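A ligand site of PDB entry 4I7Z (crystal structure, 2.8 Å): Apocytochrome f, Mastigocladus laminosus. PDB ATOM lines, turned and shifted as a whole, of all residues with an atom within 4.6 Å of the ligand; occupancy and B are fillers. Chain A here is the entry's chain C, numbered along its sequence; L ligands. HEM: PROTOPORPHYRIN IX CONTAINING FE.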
ATOM      1  N   TYR A   1     -20.308  -1.961 -20.849  1.00  0.00           N
ATOM      2  CA  TYR A   1     -20.375  -0.472 -20.988  1.00  0.00           C
ATOM      3  C   TYR A   1     -21.188   0.110 -19.837  1.00  0.00           C
ATOM      4  O   TYR A   1     -22.034  -0.579 -19.264  1.00  0.00           O
ATOM      5  CB  TYR A   1     -21.020  -0.080 -22.314  1.00  0.00           C
ATOM      6  CG  TYR A   1     -20.317  -0.635 -23.537  1.00  0.00           C
ATOM      7  CD1 TYR A   1     -20.881  -1.659 -24.276  1.00  0.00           C
ATOM      8  CD2 TYR A   1     -19.095  -0.127 -23.936  1.00  0.00           C
ATOM      9  CE1 TYR A   1     -20.236  -2.167 -25.397  1.00  0.00           C
ATOM     10  CE2 TYR A   1     -18.442  -0.629 -25.047  1.00  0.00           C
ATOM     11  CZ  TYR A   1     -19.019  -1.644 -25.770  1.00  0.00           C
ATOM     12  OH  TYR A   1     -18.357  -2.139 -26.872  1.00  0.00           O
ATOM     13  N   PRO A   2     -20.947   1.387 -19.507  1.00  0.00           N
ATOM     14  CA  PRO A   2     -21.667   2.040 -18.414  1.00  0.00           C
ATOM     15  C   PRO A   2     -23.194   1.999 -18.539  1.00  0.00           C
ATOM     16  O   PRO A   2     -23.879   2.028 -17.522  1.00  0.00           O
ATOM     17  CB  PRO A   2     -21.169   3.485 -18.473  1.00  0.00           C
ATOM     18  CG  PRO A   2     -19.844   3.411 -19.123  1.00  0.00           C
ATOM     19  CD  PRO A   2     -19.941   2.286 -20.114  1.00  0.00           C
ATOM     20  N   TRP A   4     -24.968  -0.499 -19.951  1.00  0.00           N
ATOM     21  CA  TRP A   4     -25.399  -1.863 -19.635  1.00  0.00           C
ATOM     22  C   TRP A   4     -25.615  -2.036 -18.137  1.00  0.00           C
ATOM     23  O   TRP A   4     -26.345  -2.929 -17.702  1.00  0.00           O
ATOM     24  CB  TRP A   4     -24.393  -2.886 -20.160  1.00  0.00           C
ATOM     25  CG  TRP A   4     -24.532  -3.186 -21.617  1.00  0.00           C
ATOM     26  CD1 TRP A   4     -25.615  -2.916 -22.408  1.00  0.00           C
ATOM     27  CD2 TRP A   4     -23.566  -3.806 -22.470  1.00  0.00           C
ATOM     28  NE1 TRP A   4     -25.375  -3.333 -23.697  1.00  0.00           N
ATOM     29  CE2 TRP A   4     -24.120  -3.878 -23.758  1.00  0.00           C
ATOM     30  CE3 TRP A   4     -22.270  -4.300 -22.261  1.00  0.00           C
ATOM     31  CZ2 TRP A   4     -23.432  -4.426 -24.835  1.00  0.00           C
ATOM     32  CZ3 TRP A   4     -21.596  -4.845 -23.339  1.00  0.00           C
ATOM     33  CH2 TRP A   4     -22.177  -4.906 -24.610  1.00  0.00           C
ATOM     34  N   ALA A   5     -24.975  -1.185 -17.341  1.00  0.00           N
ATOM     35  CA  ALA A   5     -25.224  -1.178 -15.911  1.00  0.00           C
ATOM     36  C   ALA A   5     -26.628  -0.643 -15.628  1.00  0.00           C
ATOM     37  O   ALA A   5     -27.343  -1.172 -14.783  1.00  0.00           O
ATOM     38  CB  ALA A   5     -24.209  -0.327 -15.210  1.00  0.00           C
ATOM     39  N   THR A   8     -28.979  -3.511 -16.877  1.00  0.00           N
ATOM     40  CA  THR A   8     -29.024  -4.682 -16.012  1.00  0.00           C
ATOM     41  C   THR A   8     -29.334  -4.324 -14.566  1.00  0.00           C
ATOM     42  O   THR A   8     -29.882  -5.138 -13.825  1.00  0.00           O
ATOM     43  CB  THR A   8     -27.689  -5.464 -16.060  1.00  0.00           C
ATOM     44  OG1 THR A   8     -27.383  -5.801 -17.421  1.00  0.00           O
ATOM     45  CG2 THR A   8     -27.773  -6.742 -15.244  1.00  0.00           C
ATOM     46  N   TYR A   9     -28.989  -3.103 -14.171  1.00  0.00           N
ATOM     47  CA  TYR A   9     -29.189  -2.653 -12.791  1.00  0.00           C
ATOM     48  C   TYR A   9     -29.765  -1.226 -12.748  1.00  0.00           C
ATOM     49  O   TYR A   9     -29.051  -0.280 -12.428  1.00  0.00           O
ATOM     50  CB  TYR A   9     -27.863  -2.725 -12.034  1.00  0.00           C
ATOM     51  CG  TYR A   9     -27.134  -4.035 -12.229  1.00  0.00           C
ATOM     52  CD1 TYR A   9     -26.152  -4.165 -13.210  1.00  0.00           C
ATOM     53  CD2 TYR A   9     -27.448  -5.147 -11.459  1.00  0.00           C
ATOM     54  CE1 TYR A   9     -25.499  -5.368 -13.406  1.00  0.00           C
ATOM     55  CE2 TYR A   9     -26.787  -6.352 -11.648  1.00  0.00           C
ATOM     56  CZ  TYR A   9     -25.816  -6.461 -12.624  1.00  0.00           C
ATOM     57  OH  TYR A   9     -25.168  -7.654 -12.811  1.00  0.00           O
ATOM     58  N   CYS A  22     -20.629  -2.893 -11.854  1.00  0.00           N
ATOM     59  CA  CYS A  22     -19.643  -2.928 -12.928  1.00  0.00           C
ATOM     60  C   CYS A  22     -18.749  -4.167 -12.849  1.00  0.00           C
ATOM     61  O   CYS A  22     -18.334  -4.713 -13.869  1.00  0.00           O
ATOM     62  CB  CYS A  22     -18.785  -1.670 -12.860  1.00  0.00           C
ATOM     63  SG  CYS A  22     -17.463  -1.560 -14.077  1.00  0.00           S
ATOM     64  N   CYS A  25     -19.069  -8.065 -14.590  1.00  0.00           N
ATOM     65  CA  CYS A  25     -18.702  -8.421 -15.959  1.00  0.00           C
ATOM     66  C   CYS A  25     -17.246  -8.124 -16.264  1.00  0.00           C
ATOM     67  O   CYS A  25     -16.601  -8.847 -17.029  1.00  0.00           O
ATOM     68  CB  CYS A  25     -19.584  -7.715 -16.960  1.00  0.00           C
ATOM     69  SG  CYS A  25     -21.300  -8.195 -16.788  1.00  0.00           S
ATOM     70  N   HIS A  26     -16.734  -7.037 -15.695  1.00  0.00           N
ATOM     71  CA  HIS A  26     -15.309  -6.741 -15.768  1.00  0.00           C
ATOM     72  C   HIS A  26     -14.623  -7.398 -14.577  1.00  0.00           C
ATOM     73  O   HIS A  26     -14.514  -6.809 -13.503  1.00  0.00           O
ATOM     74  CB  HIS A  26     -15.087  -5.228 -15.783  1.00  0.00           C
ATOM     75  CG  HIS A  26     -15.641  -4.553 -17.007  1.00  0.00           C
ATOM     76  ND1 HIS A  26     -14.903  -4.369 -18.159  1.00  0.00           N
ATOM     77  CD2 HIS A  26     -16.868  -4.039 -17.258  1.00  0.00           C
ATOM     78  CE1 HIS A  26     -15.644  -3.755 -19.058  1.00  0.00           C
ATOM     79  NE2 HIS A  26     -16.842  -3.543 -18.543  1.00  0.00           N
ATOM     80  N   GLN A  60      -5.129  -4.955 -26.483  1.00  0.00           N
ATOM     81  CA  GLN A  60      -5.960  -6.054 -26.038  1.00  0.00           C
ATOM     82  C   GLN A  60      -6.557  -6.813 -27.224  1.00  0.00           C
ATOM     83  O   GLN A  60      -6.378  -6.418 -28.379  1.00  0.00           O
ATOM     84  CB  GLN A  60      -7.100  -5.522 -25.172  1.00  0.00           C
ATOM     85  CG  GLN A  60      -8.044  -4.581 -25.901  1.00  0.00           C
ATOM     86  CD  GLN A  60      -9.149  -4.050 -25.013  1.00  0.00           C
ATOM     87  OE1 GLN A  60      -9.243  -4.413 -23.838  1.00  0.00           O
ATOM     88  NE2 GLN A  60      -9.978  -3.174 -25.562  1.00  0.00           N
ATOM     89  N   GLY A  69      -6.487  -1.049 -29.243  1.00  0.00           N
ATOM     90  CA  GLY A  69      -6.288  -0.460 -27.938  1.00  0.00           C
ATOM     91  C   GLY A  69      -7.480  -0.672 -27.030  1.00  0.00           C
ATOM     92  O   GLY A  69      -8.305  -1.552 -27.290  1.00  0.00           O
ATOM     93  N   LEU A  70      -7.585   0.128 -25.983  1.00  0.00           N
ATOM     94  CA  LEU A  70      -8.671  -0.013 -25.015  1.00  0.00           C
ATOM     95  C   LEU A  70      -9.230   1.341 -24.573  1.00  0.00           C
ATOM     96  O   LEU A  70      -8.488   2.313 -24.413  1.00  0.00           O
ATOM     97  CB  LEU A  70      -8.214  -0.825 -23.801  1.00  0.00           C
ATOM     98  CG  LEU A  70      -6.908  -0.405 -23.122  1.00  0.00           C
ATOM     99  CD1 LEU A  70      -6.913  -0.892 -21.681  1.00  0.00           C
ATOM    100  CD2 LEU A  70      -5.698  -0.975 -23.840  1.00  0.00           C
ATOM    101  N   ASN A  71     -10.545   1.391 -24.373  1.00  0.00           N
ATOM    102  CA  ASN A  71     -11.226   2.586 -23.882  1.00  0.00           C
ATOM    103  C   ASN A  71     -11.471   2.542 -22.377  1.00  0.00           C
ATOM    104  O   ASN A  71     -11.493   1.482 -21.760  1.00  0.00           O
ATOM    105  CB  ASN A  71     -12.563   2.766 -24.600  1.00  0.00           C
ATOM    106  CG  ASN A  71     -12.395   3.113 -26.051  1.00  0.00           C
ATOM    107  OD1 ASN A  71     -11.502   3.878 -26.420  1.00  0.00           O
ATOM    108  ND2 ASN A  71     -13.254   2.565 -26.902  1.00  0.00           N
ATOM    109  N   VAL A  72     -11.667   3.724 -21.789  1.00  0.00           N
ATOM    110  CA  VAL A  72     -11.947   3.844 -20.370  1.00  0.00           C
ATOM    111  C   VAL A  72     -13.397   4.231 -20.132  1.00  0.00           C
ATOM    112  O   VAL A  72     -14.019   4.874 -20.974  1.00  0.00           O
ATOM    113  CB  VAL A  72     -11.018   4.897 -19.705  1.00  0.00           C
ATOM    114  CG1 VAL A  72      -9.570   4.464 -19.801  1.00  0.00           C
ATOM    115  CG2 VAL A  72     -11.215   6.260 -20.334  1.00  0.00           C
ATOM    116  N   GLY A  73     -13.937   3.827 -18.986  1.00  0.00           N
ATOM    117  CA  GLY A  73     -15.283   4.209 -18.591  1.00  0.00           C
ATOM    118  C   GLY A  73     -15.386   4.232 -17.076  1.00  0.00           C
ATOM    119  O   GLY A  73     -14.592   3.578 -16.387  1.00  0.00           O
ATOM    120  N   ALA A  74     -16.348   4.976 -16.550  1.00  0.00           N
ATOM    121  CA  ALA A  74     -16.462   5.100 -15.098  1.00  0.00           C
ATOM    122  C   ALA A  74     -17.836   5.573 -14.624  1.00  0.00           C
ATOM    123  O   ALA A  74     -18.559   6.266 -15.350  1.00  0.00           O
ATOM    124  CB  ALA A  74     -15.381   6.027 -14.572  1.00  0.00           C
ATOM    125  N   VAL A  75     -18.174   5.178 -13.406  1.00  0.00           N
ATOM    126  CA  VAL A  75     -19.343   5.693 -12.706  1.00  0.00           C
ATOM    127  C   VAL A  75     -18.890   6.416 -11.442  1.00  0.00           C
ATOM    128  O   VAL A  75     -18.066   5.893 -10.669  1.00  0.00           O
ATOM    129  CB  VAL A  75     -20.349   4.571 -12.335  1.00  0.00           C
ATOM    130  CG1 VAL A  75     -19.666   3.450 -11.547  1.00  0.00           C
ATOM    131  CG2 VAL A  75     -21.529   5.152 -11.555  1.00  0.00           C
ATOM    132  N   VAL A 116     -19.867   7.613 -17.277  1.00  0.00           N
ATOM    133  CA  VAL A 116     -18.945   8.169 -18.249  1.00  0.00           C
ATOM    134  C   VAL A 116     -18.303   7.050 -19.059  1.00  0.00           C
ATOM    135  O   VAL A 116     -18.018   5.978 -18.522  1.00  0.00           O
ATOM    136  CB  VAL A 116     -17.862   9.002 -17.520  1.00  0.00           C
ATOM    137  CG1 VAL A 116     -16.487   8.807 -18.137  1.00  0.00           C
ATOM    138  CG2 VAL A 116     -18.251  10.470 -17.522  1.00  0.00           C
ATOM    139  N   PRO A 118     -17.931   4.943 -23.154  1.00  0.00           N
ATOM    140  CA  PRO A 118     -16.506   4.738 -23.436  1.00  0.00           C
ATOM    141  C   PRO A 118     -15.800   5.977 -23.978  1.00  0.00           C
ATOM    142  O   PRO A 118     -16.308   6.610 -24.902  1.00  0.00           O
ATOM    143  CB  PRO A 118     -16.518   3.638 -24.497  1.00  0.00           C
ATOM    144  CG  PRO A 118     -17.868   3.029 -24.436  1.00  0.00           C
ATOM    145  CD  PRO A 118     -18.778   4.134 -24.053  1.00  0.00           C
ATOM    146  N   GLY A 152     -16.206   4.153  -9.469  1.00  0.00           N
ATOM    147  CA  GLY A 152     -16.098   2.833 -10.074  1.00  0.00           C
ATOM    148  C   GLY A 152     -15.574   3.005 -11.489  1.00  0.00           C
ATOM    149  O   GLY A 152     -16.337   3.331 -12.386  1.00  0.00           O
ATOM    150  N   ASN A 154     -13.111   1.779 -14.982  1.00  0.00           N
ATOM    151  CA  ASN A 154     -12.741   0.588 -15.738  1.00  0.00           C
ATOM    152  C   ASN A 154     -12.050   0.898 -17.066  1.00  0.00           C
ATOM    153  O   ASN A 154     -12.297   1.942 -17.680  1.00  0.00           O
ATOM    154  CB  ASN A 154     -13.967  -0.284 -16.004  1.00  0.00           C
ATOM    155  CG  ASN A 154     -13.726  -1.330 -17.081  1.00  0.00           C
ATOM    156  OD1 ASN A 154     -14.082  -1.124 -18.239  1.00  0.00           O
ATOM    157  ND2 ASN A 154     -13.098  -2.431 -16.706  1.00  0.00           N
ATOM    158  N   GLY A 156     -10.692  -1.481 -20.668  1.00  0.00           N
ATOM    159  CA  GLY A 156     -10.671  -2.766 -21.349  1.00  0.00           C
ATOM    160  C   GLY A 156     -12.055  -3.347 -21.546  1.00  0.00           C
ATOM    161  O   GLY A 156     -13.029  -2.877 -20.963  1.00  0.00           O
ATOM    162  N   ARG A 157     -12.132  -4.389 -22.378  1.00  0.00           N
ATOM    163  CA  ARG A 157     -13.399  -5.049 -22.675  1.00  0.00           C
ATOM    164  C   ARG A 157     -13.817  -5.992 -21.550  1.00  0.00           C
ATOM    165  O   ARG A 157     -12.970  -6.589 -20.874  1.00  0.00           O
ATOM    166  CB  ARG A 157     -13.289  -5.837 -23.982  1.00  0.00           C
ATOM    167  CG  ARG A 157     -12.933  -4.969 -25.180  1.00  0.00           C
ATOM    168  CD  ARG A 157     -12.711  -5.812 -26.427  1.00  0.00           C
ATOM    169  NE  ARG A 157     -13.934  -6.515 -26.827  1.00  0.00           N
ATOM    170  CZ  ARG A 157     -14.005  -7.809 -27.122  1.00  0.00           C
ATOM    171  NH1 ARG A 157     -12.930  -8.592 -27.068  1.00  0.00           N
ATOM    172  NH2 ARG A 157     -15.169  -8.335 -27.476  1.00  0.00           N
ATOM    173  N   GLY A 158     -15.122  -6.128 -21.366  1.00  0.00           N
ATOM    174  CA  GLY A 158     -15.669  -6.995 -20.331  1.00  0.00           C
ATOM    175  C   GLY A 158     -15.603  -8.454 -20.724  1.00  0.00           C
ATOM    176  O   GLY A 158     -15.171  -8.784 -21.828  1.00  0.00           O
ATOM    177  N   GLN A 159     -16.033  -9.320 -19.814  1.00  0.00           N
ATOM    178  CA  GLN A 159     -15.946 -10.767 -20.021  1.00  0.00           C
ATOM    179  C   GLN A 159     -17.313 -11.411 -20.188  1.00  0.00           C
ATOM    180  O   GLN A 159     -17.415 -12.530 -20.698  1.00  0.00           O
ATOM    181  CB  GLN A 159     -15.215 -11.416 -18.854  1.00  0.00           C
ATOM    182  CG  GLN A 159     -13.718 -11.189 -18.867  1.00  0.00           C
ATOM    183  CD  GLN A 159     -13.333  -9.749 -18.621  1.00  0.00           C
ATOM    184  OE1 GLN A 159     -13.715  -9.144 -17.607  1.00  0.00           O
ATOM    185  NE2 GLN A 159     -12.580  -9.176 -19.540  1.00  0.00           N
ATOM    186  N   ILE A 160     -18.360 -10.712 -19.758  1.00  0.00           N
ATOM    187  CA  ILE A 160     -19.719 -11.223 -19.835  1.00  0.00           C
ATOM    188  C   ILE A 160     -20.678 -10.188 -20.426  1.00  0.00           C
ATOM    189  O   ILE A 160     -20.597  -8.999 -20.097  1.00  0.00           O
ATOM    190  CB  ILE A 160     -20.234 -11.632 -18.440  1.00  0.00           C
ATOM    191  CG1 ILE A 160     -19.196 -12.492 -17.722  1.00  0.00           C
ATOM    192  CG2 ILE A 160     -21.563 -12.384 -18.573  1.00  0.00           C
ATOM    193  CD1 ILE A 160     -19.547 -12.823 -16.292  1.00  0.00           C
ATOM    194  N   TYR A 161     -21.570 -10.640 -21.307  1.00  0.00           N
ATOM    195  CA  TYR A 161     -22.563  -9.762 -21.916  1.00  0.00           C
ATOM    196  C   TYR A 161     -23.859  -9.754 -21.106  1.00  0.00           C
ATOM    197  O   TYR A 161     -24.086 -10.659 -20.303  1.00  0.00           O
ATOM    198  CB  TYR A 161     -22.858 -10.209 -23.345  1.00  0.00           C
ATOM    199  CG  TYR A 161     -21.703 -10.043 -24.296  1.00  0.00           C
ATOM    200  CD1 TYR A 161     -20.954 -11.134 -24.706  1.00  0.00           C
ATOM    201  CD2 TYR A 161     -21.354  -8.789 -24.781  1.00  0.00           C
ATOM    202  CE1 TYR A 161     -19.906 -10.999 -25.583  1.00  0.00           C
ATOM    203  CE2 TYR A 161     -20.295  -8.634 -25.660  1.00  0.00           C
ATOM    204  CZ  TYR A 161     -19.572  -9.746 -26.056  1.00  0.00           C
ATOM    205  OH  TYR A 161     -18.510  -9.614 -26.932  1.00  0.00           O
ATOM    206  N   PRO A 162     -24.703  -8.729 -21.321  1.00  0.00           N
ATOM    207  CA  PRO A 162     -25.967  -8.627 -20.574  1.00  0.00           C
ATOM    208  C   PRO A 162     -26.878  -9.832 -20.771  1.00  0.00           C
ATOM    209  O   PRO A 162     -27.697 -10.129 -19.906  1.00  0.00           O
ATOM    210  CB  PRO A 162     -26.623  -7.381 -21.177  1.00  0.00           C
ATOM    211  CG  PRO A 162     -25.492  -6.582 -21.714  1.00  0.00           C
ATOM    212  CD  PRO A 162     -24.496  -7.581 -22.205  1.00  0.00           C
HETATM  213  CHA HEM L   1     -17.135  -2.730 -22.698  1.00  0.00           C
HETATM  214  CHB HEM L   1     -16.810   0.297 -18.909  1.00  0.00           C
HETATM  215  CHC HEM L   1     -20.430  -2.070 -16.714  1.00  0.00           C
HETATM  216  CHD HEM L   1     -19.751  -5.711 -19.866  1.00  0.00           C
HETATM  217  C1A HEM L   1     -16.781  -1.666 -21.889  1.00  0.00           C
HETATM  218  C2A HEM L   1     -15.866  -0.609 -22.230  1.00  0.00           C
HETATM  219  C3A HEM L   1     -15.778   0.224 -21.193  1.00  0.00           C
HETATM  220  C4A HEM L   1     -16.635  -0.279 -20.146  1.00  0.00           C
HETATM  221  CMA HEM L   1     -14.929   1.515 -21.087  1.00  0.00           C
HETATM  222  CAA HEM L   1     -15.136  -0.487 -23.587  1.00  0.00           C
HETATM  223  CBA HEM L   1     -13.650  -0.759 -23.393  1.00  0.00           C
HETATM  224  CGA HEM L   1     -12.973  -0.937 -24.724  1.00  0.00           C
HETATM  225  O1A HEM L   1     -13.663  -0.867 -25.781  1.00  0.00           O
HETATM  226  O2A HEM L   1     -11.731  -1.141 -24.718  1.00  0.00           O
HETATM  227  C1B HEM L   1     -17.806  -0.029 -18.017  1.00  0.00           C
HETATM  228  C2B HEM L   1     -18.197   0.743 -16.869  1.00  0.00           C
HETATM  229  C3B HEM L   1     -19.206   0.115 -16.262  1.00  0.00           C
HETATM  230  C4B HEM L   1     -19.483  -1.116 -16.998  1.00  0.00           C
HETATM  231  CMB HEM L   1     -17.594   2.091 -16.407  1.00  0.00           C
HETATM  232  CAB HEM L   1     -19.902   0.635 -14.988  1.00  0.00           C
HETATM  233  CBB HEM L   1     -21.073   0.124 -14.610  1.00  0.00           C
HETATM  234  C1C HEM L   1     -20.629  -3.231 -17.451  1.00  0.00           C
HETATM  235  C2C HEM L   1     -21.781  -4.105 -17.385  1.00  0.00           C
HETATM  236  C3C HEM L   1     -21.598  -5.099 -18.256  1.00  0.00           C
HETATM  237  C4C HEM L   1     -20.320  -4.903 -18.909  1.00  0.00           C
HETATM  238  CMC HEM L   1     -23.006  -3.889 -16.455  1.00  0.00           C
HETATM  239  CAC HEM L   1     -22.547  -6.276 -18.580  1.00  0.00           C
HETATM  240  CBC HEM L   1     -23.703  -6.472 -17.928  1.00  0.00           C
HETATM  241  C1D HEM L   1     -19.007  -5.283 -20.952  1.00  0.00           C
HETATM  242  C2D HEM L   1     -18.674  -6.057 -22.133  1.00  0.00           C
HETATM  243  C3D HEM L   1     -17.849  -5.111 -23.008  1.00  0.00           C
HETATM  244  C4D HEM L   1     -17.780  -3.875 -22.276  1.00  0.00           C
HETATM  245  CMD HEM L   1     -19.049  -7.531 -22.459  1.00  0.00           C
HETATM  246  CAD HEM L   1     -17.243  -5.410 -24.394  1.00  0.00           C
HETATM  247  CBD HEM L   1     -18.326  -6.014 -25.286  1.00  0.00           C
HETATM  248  CGD HEM L   1     -17.795  -6.044 -26.692  1.00  0.00           C
HETATM  249  O1D HEM L   1     -18.500  -6.539 -27.609  1.00  0.00           O
HETATM  250  O2D HEM L   1     -16.640  -5.577 -26.885  1.00  0.00           O
HETATM  251  NA  HEM L   1     -17.227  -1.444 -20.600  1.00  0.00           N
HETATM  252  NB  HEM L   1     -18.600  -1.166 -18.068  1.00  0.00           N
HETATM  253  NC  HEM L   1     -19.759  -3.751 -18.387  1.00  0.00           N
HETATM  254  ND  HEM L   1     -18.468  -4.016 -21.081  1.00  0.00           N
HETATM  255 FE   HEM L   1     -18.575  -2.624 -19.599  1.00  0.00          FE
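A ring nitrogen (ND1) of His 26 lies within hydrogen-bond range of the side-chain amide nitrogen (ND2) of Asn 154 (3.0 Å). The side-chain amide oxygen (OE1) of Gln 60 is in hydrogen-bond range of the backbone NH (N) of Arg 157 (3.2 Å). The backbone carbonyl oxygen (O) of Gly 69 sits at hydrogen-bond distance from the side-chain amide nitrogen (NE2) of Gln 60, 2.9 Å away. The backbone carbonyl oxygen (O) of Asn 71 is in hydrogen-bond range of the backbone NH (N) of Gly 156. The side-chain amide nitrogen (NE2) of Gln 159 lies within hydrogen-bond range of the backbone carbonyl oxygen (O) of Arg 157, 2.9 Å away. The side-chain sulfur of Cys 25 sits at hydrogen-bond distance from the backbone carbonyl oxygen of Ile 160 (3.5 Å). The backbone carbonyl oxygen (O) of Cys 25 lies within hydrogen-bond range of the backbone NH (N) of Gln 159, at 2.9 Å. The side-chain amide oxygen (OD1) of Asn 154 lies close to the backbone carbonyl oxygen (O) of Gly 156 (3.4 Å).
A ring nitrogen (NE2) of His 26 binds an iron atom (FE) of the ligand, 2.2 Å away. N of Tyr 1 is bound to FE of the ligand (2.2 Å). O2A of the ligand lies within hydrogen-bond range of NE2 of Gln 60 (2.8 Å). The backbone NH (N) of Asn 71 lies within hydrogen-bond range of an oxygen (O2A) of the ligand (2.8 Å). O2D of the ligand lies within salt-bridge range of NE of Arg 157, at 2.9 Å. An oxygen (O1D) of the ligand lies within hydrogen-bond range of the side-chain hydroxyl (OH) of Tyr 161.
Pro 2 touches the ligand. CZ3 of Trp 4 touches C2D of the ligand (3.4 Å). Ala 5 touches the ligand. Thr 8 touches the ligand. Cys 22 touches the ligand (SG to C3B, 3.3 Å). Cys 25 touches the ligand (SG to CAC, 2.9 Å). CA of Leu 70 touches O2A of the ligand (3.3 Å). C of Val 72 touches CMA of the ligand, 3.3 Å away. Gly 73 touches the ligand (C to CMB, 3.1 Å). N of Ala 74 touches CMB of the ligand, at 3.1 Å. Asn 154 touches the ligand. Gly 156 touches the ligand. Gly 158 touches the ligand. O of Ile 160 touches CMD of the ligand (3.2 Å). 20 residues have an atom within 4 Å of the ligand: Tyr 1, Pro 2, Trp 4, Ala 5, Thr 8, Cys 22, Cys 25, His 26, Gln 60, Leu 70, Asn 71, Val 72, Gly 73, Ala 74, Asn 154, Gly 156, Arg 157, Gly 158, Ile 160 and Tyr 161. The nearest printed residue that does not touch the ligand is Pro 162 (4.1 Å).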
